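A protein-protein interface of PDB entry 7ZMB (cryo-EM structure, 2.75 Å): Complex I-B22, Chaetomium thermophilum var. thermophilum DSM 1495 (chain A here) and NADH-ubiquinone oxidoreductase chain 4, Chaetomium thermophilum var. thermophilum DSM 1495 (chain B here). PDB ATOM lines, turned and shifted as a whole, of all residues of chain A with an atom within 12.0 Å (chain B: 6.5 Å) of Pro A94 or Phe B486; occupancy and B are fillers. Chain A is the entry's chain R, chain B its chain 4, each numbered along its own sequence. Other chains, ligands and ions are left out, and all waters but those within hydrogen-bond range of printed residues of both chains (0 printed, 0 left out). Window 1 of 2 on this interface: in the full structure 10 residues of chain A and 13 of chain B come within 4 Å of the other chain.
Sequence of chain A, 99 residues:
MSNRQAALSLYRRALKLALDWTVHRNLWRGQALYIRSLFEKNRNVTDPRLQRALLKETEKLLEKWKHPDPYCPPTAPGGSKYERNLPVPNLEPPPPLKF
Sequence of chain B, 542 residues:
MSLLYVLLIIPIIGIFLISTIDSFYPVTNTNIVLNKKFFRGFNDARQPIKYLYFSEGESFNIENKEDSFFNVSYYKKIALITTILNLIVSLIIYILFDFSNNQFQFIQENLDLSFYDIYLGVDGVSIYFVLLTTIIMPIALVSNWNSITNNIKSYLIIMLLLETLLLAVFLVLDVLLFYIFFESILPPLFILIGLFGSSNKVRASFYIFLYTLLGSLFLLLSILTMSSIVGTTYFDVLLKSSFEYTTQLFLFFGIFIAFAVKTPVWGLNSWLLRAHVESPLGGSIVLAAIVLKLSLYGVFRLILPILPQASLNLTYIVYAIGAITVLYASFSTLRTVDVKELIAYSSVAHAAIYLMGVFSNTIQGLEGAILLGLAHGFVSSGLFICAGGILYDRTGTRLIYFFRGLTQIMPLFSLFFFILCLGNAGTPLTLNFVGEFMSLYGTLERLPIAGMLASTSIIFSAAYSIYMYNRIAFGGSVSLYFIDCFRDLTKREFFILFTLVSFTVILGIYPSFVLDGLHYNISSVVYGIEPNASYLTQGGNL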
ATOM      1  N   VAL A  88     -12.116   3.177   8.162  1.00  0.00           N
ATOM      2  CA  VAL A  88     -10.820   3.029   7.494  1.00  0.00           C
ATOM      3  C   VAL A  88     -10.826   3.853   6.212  1.00  0.00           C
ATOM      4  O   VAL A  88     -11.846   3.883   5.500  1.00  0.00           O
ATOM      5  CB  VAL A  88     -10.521   1.555   7.216  1.00  0.00           C
ATOM      6  CG1 VAL A  88     -10.756   0.728   8.468  1.00  0.00           C
ATOM      7  CG2 VAL A  88     -11.317   1.039   6.039  1.00  0.00           C
ATOM      8  N   PRO A  89      -9.760   4.586   5.913  1.00  0.00           N
ATOM      9  CA  PRO A  89      -9.762   5.413   4.697  1.00  0.00           C
ATOM     10  C   PRO A  89      -9.879   4.613   3.411  1.00  0.00           C
ATOM     11  O   PRO A  89     -10.301   5.166   2.388  1.00  0.00           O
ATOM     12  CB  PRO A  89      -8.420   6.151   4.780  1.00  0.00           C
ATOM     13  CG  PRO A  89      -8.105   6.175   6.242  1.00  0.00           C
ATOM     14  CD  PRO A  89      -8.624   4.888   6.794  1.00  0.00           C
ATOM     15  N   ASN A  90      -9.522   3.332   3.430  1.00  0.00           N
ATOM     16  CA  ASN A  90      -9.449   2.506   2.231  1.00  0.00           C
ATOM     17  C   ASN A  90     -10.334   1.285   2.435  1.00  0.00           C
ATOM     18  O   ASN A  90      -9.966   0.361   3.169  1.00  0.00           O
ATOM     19  CB  ASN A  90      -7.999   2.111   1.953  1.00  0.00           C
ATOM     20  CG  ASN A  90      -7.840   1.306   0.694  1.00  0.00           C
ATOM     21  OD1 ASN A  90      -8.767   1.172  -0.090  1.00  0.00           O
ATOM     22  ND2 ASN A  90      -6.647   0.775   0.485  1.00  0.00           N
ATOM     23  N   LEU A  91     -11.495   1.276   1.783  1.00  0.00           N
ATOM     24  CA  LEU A  91     -12.444   0.182   1.939  1.00  0.00           C
ATOM     25  C   LEU A  91     -12.188  -0.986   1.003  1.00  0.00           C
ATOM     26  O   LEU A  91     -12.754  -2.061   1.223  1.00  0.00           O
ATOM     27  CB  LEU A  91     -13.877   0.678   1.721  1.00  0.00           C
ATOM     28  CG  LEU A  91     -14.616   1.343   2.883  1.00  0.00           C
ATOM     29  CD1 LEU A  91     -14.815   0.341   4.010  1.00  0.00           C
ATOM     30  CD2 LEU A  91     -13.894   2.582   3.384  1.00  0.00           C
ATOM     31  N   GLU A  92     -11.375  -0.810  -0.027  1.00  0.00           N
ATOM     32  CA  GLU A  92     -11.189  -1.891  -0.985  1.00  0.00           C
ATOM     33  C   GLU A  92     -10.268  -2.968  -0.412  1.00  0.00           C
ATOM     34  O   GLU A  92      -9.314  -2.655   0.305  1.00  0.00           O
ATOM     35  CB  GLU A  92     -10.629  -1.353  -2.296  1.00  0.00           C
ATOM     36  CG  GLU A  92     -11.598  -0.458  -3.064  1.00  0.00           C
ATOM     37  CD  GLU A  92     -11.613   0.976  -2.574  1.00  0.00           C
ATOM     38  OE1 GLU A  92     -10.824   1.308  -1.669  1.00  0.00           O
ATOM     39  OE2 GLU A  92     -12.412   1.777  -3.103  1.00  0.00           O
ATOM     40  N   PRO A  93     -10.534  -4.241  -0.718  1.00  0.00           N
ATOM     41  CA  PRO A  93      -9.737  -5.317  -0.129  1.00  0.00           C
ATOM     42  C   PRO A  93      -8.321  -5.311  -0.675  1.00  0.00           C
ATOM     43  O   PRO A  93      -8.066  -4.806  -1.781  1.00  0.00           O
ATOM     44  CB  PRO A  93     -10.492  -6.591  -0.551  1.00  0.00           C
ATOM     45  CG  PRO A  93     -11.822  -6.124  -1.080  1.00  0.00           C
ATOM     46  CD  PRO A  93     -11.595  -4.751  -1.602  1.00  0.00           C
ATOM     47  N   PRO A  94      -7.358  -5.856   0.074  1.00  0.00           N
ATOM     48  CA  PRO A  94      -5.978  -5.860  -0.399  1.00  0.00           C
ATOM     49  C   PRO A  94      -5.812  -6.754  -1.613  1.00  0.00           C
ATOM     50  O   PRO A  94      -6.503  -7.778  -1.749  1.00  0.00           O
ATOM     51  CB  PRO A  94      -5.194  -6.403   0.811  1.00  0.00           C
ATOM     52  CG  PRO A  94      -6.077  -6.128   1.973  1.00  0.00           C
ATOM     53  CD  PRO A  94      -7.460  -6.341   1.458  1.00  0.00           C
ATOM     54  N   PRO A  95      -4.884  -6.426  -2.506  1.00  0.00           N
ATOM     55  CA  PRO A  95      -4.743  -7.171  -3.757  1.00  0.00           C
ATOM     56  C   PRO A  95      -4.033  -8.493  -3.532  1.00  0.00           C
ATOM     57  O   PRO A  95      -3.450  -8.718  -2.462  1.00  0.00           O
ATOM     58  CB  PRO A  95      -3.892  -6.226  -4.616  1.00  0.00           C
ATOM     59  CG  PRO A  95      -3.029  -5.561  -3.625  1.00  0.00           C
ATOM     60  CD  PRO A  95      -3.885  -5.351  -2.404  1.00  0.00           C
ATOM     61  N   PRO A  96      -4.045  -9.388  -4.517  1.00  0.00           N
ATOM     62  CA  PRO A  96      -3.375 -10.680  -4.330  1.00  0.00           C
ATOM     63  C   PRO A  96      -1.861 -10.560  -4.300  1.00  0.00           C
ATOM     64  O   PRO A  96      -1.222 -10.338  -5.332  1.00  0.00           O
ATOM     65  CB  PRO A  96      -3.847 -11.496  -5.540  1.00  0.00           C
ATOM     66  CG  PRO A  96      -4.189 -10.479  -6.568  1.00  0.00           C
ATOM     67  CD  PRO A  96      -4.747  -9.314  -5.811  1.00  0.00           C
ATOM     68  N   LEU A  97      -1.281 -10.706  -3.112  1.00  0.00           N
ATOM     69  CA  LEU A  97       0.162 -10.725  -2.938  1.00  0.00           C
ATOM     70  C   LEU A  97       0.543 -11.891  -2.043  1.00  0.00           C
ATOM     71  O   LEU A  97      -0.204 -12.267  -1.137  1.00  0.00           O
ATOM     72  CB  LEU A  97       0.683  -9.418  -2.336  1.00  0.00           C
ATOM     73  CG  LEU A  97       0.957  -8.280  -3.318  1.00  0.00           C
ATOM     74  CD1 LEU A  97       1.687  -7.153  -2.631  1.00  0.00           C
ATOM     75  CD2 LEU A  97       1.754  -8.786  -4.500  1.00  0.00           C
ATOM     76  N   LYS A  98       1.711 -12.461  -2.305  1.00  0.00           N
ATOM     77  CA  LYS A  98       2.236 -13.572  -1.515  1.00  0.00           C
ATOM     78  C   LYS A  98       3.185 -13.000  -0.469  1.00  0.00           C
ATOM     79  O   LYS A  98       4.317 -12.621  -0.782  1.00  0.00           O
ATOM     80  CB  LYS A  98       2.928 -14.598  -2.406  1.00  0.00           C
ATOM     81  CG  LYS A  98       1.989 -15.595  -3.068  1.00  0.00           C
ATOM     82  CD  LYS A  98       1.188 -14.965  -4.198  1.00  0.00           C
ATOM     83  CE  LYS A  98       2.079 -14.627  -5.379  1.00  0.00           C
ATOM     84  NZ  LYS A  98       1.299 -14.067  -6.517  1.00  0.00           N
ATOM     85  N   PHE A  99       2.720 -12.937   0.774  1.00  0.00           N
ATOM     86  CA  PHE A  99       3.529 -12.433   1.876  1.00  0.00           C
ATOM     87  C   PHE A  99       3.739 -13.509   2.935  1.00  0.00           C
ATOM     88  O   PHE A  99       4.669 -13.430   3.736  1.00  0.00           O
ATOM     89  CB  PHE A  99       2.876 -11.199   2.502  1.00  0.00           C
ATOM     90  CG  PHE A  99       3.164  -9.933   1.763  1.00  0.00           C
ATOM     91  CD1 PHE A  99       4.451  -9.623   1.379  1.00  0.00           C
ATOM     92  CD2 PHE A  99       2.149  -9.058   1.433  1.00  0.00           C
ATOM     93  CE1 PHE A  99       4.719  -8.464   0.694  1.00  0.00           C
ATOM     94  CE2 PHE A  99       2.416  -7.902   0.744  1.00  0.00           C
ATOM     95  CZ  PHE A  99       3.696  -7.603   0.376  1.00  0.00           C
ATOM     96  N   LEU B 391       6.069  -5.464   8.763  1.00  0.00           N
ATOM     97  CA  LEU B 391       5.929  -4.135   8.185  1.00  0.00           C
ATOM     98  C   LEU B 391       6.804  -3.968   6.952  1.00  0.00           C
ATOM     99  O   LEU B 391       6.337  -3.509   5.906  1.00  0.00           O
ATOM    100  CB  LEU B 391       6.285  -3.070   9.218  1.00  0.00           C
ATOM    101  CG  LEU B 391       5.664  -3.159  10.602  1.00  0.00           C
ATOM    102  CD1 LEU B 391       6.004  -1.900  11.356  1.00  0.00           C
ATOM    103  CD2 LEU B 391       4.170  -3.353  10.503  1.00  0.00           C
ATOM    104  N   ARG B 394       5.575  -5.690   3.796  1.00  0.00           N
ATOM    105  CA  ARG B 394       4.398  -5.109   3.164  1.00  0.00           C
ATOM    106  C   ARG B 394       4.677  -3.734   2.577  1.00  0.00           C
ATOM    107  O   ARG B 394       4.132  -3.391   1.526  1.00  0.00           O
ATOM    108  CB  ARG B 394       3.252  -5.036   4.166  1.00  0.00           C
ATOM    109  CG  ARG B 394       2.663  -6.381   4.497  1.00  0.00           C
ATOM    110  CD  ARG B 394       1.841  -6.310   5.755  1.00  0.00           C
ATOM    111  NE  ARG B 394       1.069  -7.526   5.992  1.00  0.00           N
ATOM    112  CZ  ARG B 394       1.589  -8.692   6.355  1.00  0.00           C
ATOM    113  NH1 ARG B 394       0.804  -9.736   6.549  1.00  0.00           N
ATOM    114  NH2 ARG B 394       2.889  -8.818   6.534  1.00  0.00           N
ATOM    115  N   THR B 395       5.514  -2.932   3.230  1.00  0.00           N
ATOM    116  CA  THR B 395       5.650  -1.530   2.866  1.00  0.00           C
ATOM    117  C   THR B 395       6.962  -1.182   2.189  1.00  0.00           C
ATOM    118  O   THR B 395       7.049  -0.121   1.567  1.00  0.00           O
ATOM    119  CB  THR B 395       5.491  -0.644   4.106  1.00  0.00           C
ATOM    120  OG1 THR B 395       6.676  -0.722   4.904  1.00  0.00           O
ATOM    121  CG2 THR B 395       4.308  -1.095   4.918  1.00  0.00           C
ATOM    122  N   PHE B 403       3.731   4.932   9.240  1.00  0.00           N
ATOM    123  CA  PHE B 403       2.876   3.974   9.918  1.00  0.00           C
ATOM    124  C   PHE B 403       2.054   4.683  10.977  1.00  0.00           C
ATOM    125  O   PHE B 403       2.559   5.545  11.699  1.00  0.00           O
ATOM    126  CB  PHE B 403       3.678   2.849  10.557  1.00  0.00           C
ATOM    127  CG  PHE B 403       4.536   2.097   9.593  1.00  0.00           C
ATOM    128  CD1 PHE B 403       4.046   0.991   8.933  1.00  0.00           C
ATOM    129  CD2 PHE B 403       5.834   2.497   9.347  1.00  0.00           C
ATOM    130  CE1 PHE B 403       4.838   0.302   8.047  1.00  0.00           C
ATOM    131  CE2 PHE B 403       6.625   1.816   8.460  1.00  0.00           C
ATOM    132  CZ  PHE B 403       6.134   0.718   7.811  1.00  0.00           C
ATOM    133  N   LEU B 406      -2.535   0.877  12.491  1.00  0.00           N
ATOM    134  CA  LEU B 406      -2.691  -0.403  11.819  1.00  0.00           C
ATOM    135  C   LEU B 406      -3.692  -1.315  12.497  1.00  0.00           C
ATOM    136  O   LEU B 406      -4.107  -2.308  11.892  1.00  0.00           O
ATOM    137  CB  LEU B 406      -1.353  -1.135  11.697  1.00  0.00           C
ATOM    138  CG  LEU B 406      -0.333  -0.517  10.760  1.00  0.00           C
ATOM    139  CD1 LEU B 406       0.962  -1.278  10.826  1.00  0.00           C
ATOM    140  CD2 LEU B 406      -0.889  -0.545   9.363  1.00  0.00           C
ATOM    141  N   ILE B 409      -6.748  -2.475  10.611  1.00  0.00           N
ATOM    142  CA  ILE B 409      -6.632  -3.307   9.421  1.00  0.00           C
ATOM    143  C   ILE B 409      -5.957  -4.624   9.782  1.00  0.00           C
ATOM    144  O   ILE B 409      -6.174  -5.647   9.123  1.00  0.00           O
ATOM    145  CB  ILE B 409      -5.875  -2.541   8.316  1.00  0.00           C
ATOM    146  CG1 ILE B 409      -6.795  -1.511   7.693  1.00  0.00           C
ATOM    147  CG2 ILE B 409      -5.407  -3.457   7.211  1.00  0.00           C
ATOM    148  CD1 ILE B 409      -8.027  -2.118   7.074  1.00  0.00           C
ATOM    149  N   MET B 410      -5.180  -4.621  10.863  1.00  0.00           N
ATOM    150  CA  MET B 410      -4.396  -5.781  11.289  1.00  0.00           C
ATOM    151  C   MET B 410      -4.722  -6.094  12.742  1.00  0.00           C
ATOM    152  O   MET B 410      -3.962  -5.734  13.648  1.00  0.00           O
ATOM    153  CB  MET B 410      -2.901  -5.512  11.139  1.00  0.00           C
ATOM    154  CG  MET B 410      -2.394  -5.359   9.721  1.00  0.00           C
ATOM    155  SD  MET B 410      -0.634  -5.039   9.808  1.00  0.00           S
ATOM    156  CE  MET B 410      -0.226  -4.795   8.099  1.00  0.00           C
ATOM    157  N   PHE B 482      -0.595   4.780   2.743  1.00  0.00           N
ATOM    158  CA  PHE B 482      -0.943   3.466   2.209  1.00  0.00           C
ATOM    159  C   PHE B 482      -1.963   3.666   1.104  1.00  0.00           C
ATOM    160  O   PHE B 482      -3.146   3.884   1.370  1.00  0.00           O
ATOM    161  CB  PHE B 482      -1.511   2.553   3.292  1.00  0.00           C
ATOM    162  CG  PHE B 482      -0.602   2.345   4.461  1.00  0.00           C
ATOM    163  CD1 PHE B 482       0.765   2.357   4.308  1.00  0.00           C
ATOM    164  CD2 PHE B 482      -1.119   2.131   5.720  1.00  0.00           C
ATOM    165  CE1 PHE B 482       1.596   2.159   5.382  1.00  0.00           C
ATOM    166  CE2 PHE B 482      -0.288   1.936   6.797  1.00  0.00           C
ATOM    167  CZ  PHE B 482       1.070   1.945   6.624  1.00  0.00           C
ATOM    168  N   ILE B 483      -1.519   3.583  -0.147  1.00  0.00           N
ATOM    169  CA  ILE B 483      -2.446   3.699  -1.264  1.00  0.00           C
ATOM    170  C   ILE B 483      -2.978   2.314  -1.610  1.00  0.00           C
ATOM    171  O   ILE B 483      -3.605   2.118  -2.656  1.00  0.00           O
ATOM    172  CB  ILE B 483      -1.788   4.372  -2.479  1.00  0.00           C
ATOM    173  CG1 ILE B 483      -0.826   3.423  -3.172  1.00  0.00           C
ATOM    174  CG2 ILE B 483      -1.069   5.635  -2.054  1.00  0.00           C
ATOM    175  CD1 ILE B 483      -0.049   4.061  -4.293  1.00  0.00           C
ATOM    176  N   ASP B 484      -2.752   1.353  -0.722  1.00  0.00           N
ATOM    177  CA  ASP B 484      -3.198  -0.012  -0.960  1.00  0.00           C
ATOM    178  C   ASP B 484      -3.398  -0.695   0.385  1.00  0.00           C
ATOM    179  O   ASP B 484      -2.491  -0.691   1.219  1.00  0.00           O
ATOM    180  CB  ASP B 484      -2.178  -0.757  -1.814  1.00  0.00           C
ATOM    181  CG  ASP B 484      -2.740  -2.003  -2.426  1.00  0.00           C
ATOM    182  OD1 ASP B 484      -3.932  -2.285  -2.197  1.00  0.00           O
ATOM    183  OD2 ASP B 484      -1.990  -2.690  -3.146  1.00  0.00           O
ATOM    184  N   CYS B 485      -4.577  -1.274   0.596  1.00  0.00           N
ATOM    185  CA  CYS B 485      -4.906  -1.857   1.889  1.00  0.00           C
ATOM    186  C   CYS B 485      -4.029  -3.076   2.157  1.00  0.00           C
ATOM    187  O   CYS B 485      -3.538  -3.730   1.232  1.00  0.00           O
ATOM    188  CB  CYS B 485      -6.390  -2.230   1.937  1.00  0.00           C
ATOM    189  SG  CYS B 485      -7.045  -2.617   3.584  1.00  0.00           S
ATOM    190  N   PHE B 486      -3.808  -3.365   3.436  1.00  0.00           N
ATOM    191  CA  PHE B 486      -2.851  -4.384   3.849  1.00  0.00           C
ATOM    192  C   PHE B 486      -3.561  -5.647   4.308  1.00  0.00           C
ATOM    193  O   PHE B 486      -4.579  -5.583   5.000  1.00  0.00           O
ATOM    194  CB  PHE B 486      -1.963  -3.889   4.993  1.00  0.00           C
ATOM    195  CG  PHE B 486      -0.967  -2.849   4.590  1.00  0.00           C
ATOM    196  CD1 PHE B 486      -0.830  -2.472   3.270  1.00  0.00           C
ATOM    197  CD2 PHE B 486      -0.157  -2.257   5.539  1.00  0.00           C
ATOM    198  CE1 PHE B 486       0.085  -1.522   2.904  1.00  0.00           C
ATOM    199  CE2 PHE B 486       0.763  -1.307   5.178  1.00  0.00           C
ATOM    200  CZ  PHE B 486       0.889  -0.941   3.854  1.00  0.00           C
ATOM    201  N   ARG B 487      -3.012  -6.794   3.935  1.00  0.00           N
ATOM    202  CA  ARG B 487      -3.447  -8.037   4.545  1.00  0.00           C
ATOM    203  C   ARG B 487      -2.888  -8.143   5.956  1.00  0.00           C
ATOM    204  O   ARG B 487      -1.838  -7.583   6.278  1.00  0.00           O
ATOM    205  CB  ARG B 487      -3.004  -9.238   3.718  1.00  0.00           C
ATOM    206  CG  ARG B 487      -1.508  -9.460   3.690  1.00  0.00           C
ATOM    207  CD  ARG B 487      -1.168 -10.711   2.916  1.00  0.00           C
ATOM    208  NE  ARG B 487      -2.088 -11.799   3.224  1.00  0.00           N
ATOM    209  CZ  ARG B 487      -2.100 -12.966   2.591  1.00  0.00           C
ATOM    210  NH1 ARG B 487      -2.971 -13.901   2.938  1.00  0.00           N
ATOM    211  NH2 ARG B 487      -1.240 -13.196   1.613  1.00  0.00           N
ATOM    212  N   ASP B 488      -3.606  -8.876   6.800  1.00  0.00           N
ATOM    213  CA  ASP B 488      -3.196  -9.088   8.180  1.00  0.00           C
ATOM    214  C   ASP B 488      -2.102 -10.144   8.236  1.00  0.00           C
ATOM    215  O   ASP B 488      -1.495 -10.470   7.213  1.00  0.00           O
ATOM    216  CB  ASP B 488      -4.396  -9.506   9.037  1.00  0.00           C
ATOM    217  CG  ASP B 488      -4.151  -9.322  10.522  1.00  0.00           C
ATOM    218  OD1 ASP B 488      -3.023  -8.947  10.887  1.00  0.00           O
ATOM    219  OD2 ASP B 488      -5.070  -9.574  11.324  1.00  0.00           O
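The backbone NH (N) of Cys B485 lies close to the side-chain amide nitrogen (ND2) of Asn A90.
The backbone carbonyl oxygen (O) of Leu A97 sits at hydrogen-bond distance from the guanidinium group (NH2) of Arg B487, 3.1 Å away.
OD1 of Asn A90 sits close to OE1 of Glu A92 (2.6 Å).
O of Arg B487 lies within hydrogen-bond range of NE of Arg B394, at 2.9 Å.
O of Asp B488 is in hydrogen-bond range of NH1 of Arg B394, 2.5 Å away.
Asp B484 touches Asn A90 (C to ND2, 3.6 Å).
Glu A92 touches Cys B485 (O to CB, 3.4 Å).
Cys B485 touches Pro A94.
Pro A94 touches Phe B486.
Arg B487 touches Pro A94 (N to CG, 3.7 Å).
Pro A95 touches Asp B484.
Pro A95 touches Cys B485 (CD to O, 3.996 Å).
Arg B394 touches Phe A99 (CA to CZ, 3.8 Å).
CD2 of Phe A99 touches CD of Arg B487, 3.99 Å away.
Pro A94 touches just these residues of chain B: Cys B485, Phe B486 and Arg B487.
Phe B486 touches just one residue of chain A: Pro A94.
Of chain A, only Phe A99 comes within 4 Å of Arg B394.
No residue of chain A comes within 4 Å of Thr B395.
No residue of chain A comes within 4 Å of Phe B482.
Asp B488 touches none of the printed residues of chain A.
Printed residues of chain B within 4 Å of Asn A90: Asp B484 and Cys B485.
Of the printed residues of chain B, Phe A99 touches Arg B394 and Arg B487.
The nearest residue of chain B that does not touch Pro A94 is Asp B484 (4.5 Å).
Of the 12 printed residues of chain A, 6 touch a printed residue of chain B.
Hydrophobic or aromatic side chains of chain A within 4 Å of the printed part of chain B: Pro A94, Pro A95 and Phe A99.
Among the printed residues, 11 pairs touch across the chains.
Among the printed residues, no Asp or Glu carboxylate lies within 4 Å of a Lys or Arg side-chain nitrogen of the other chain.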
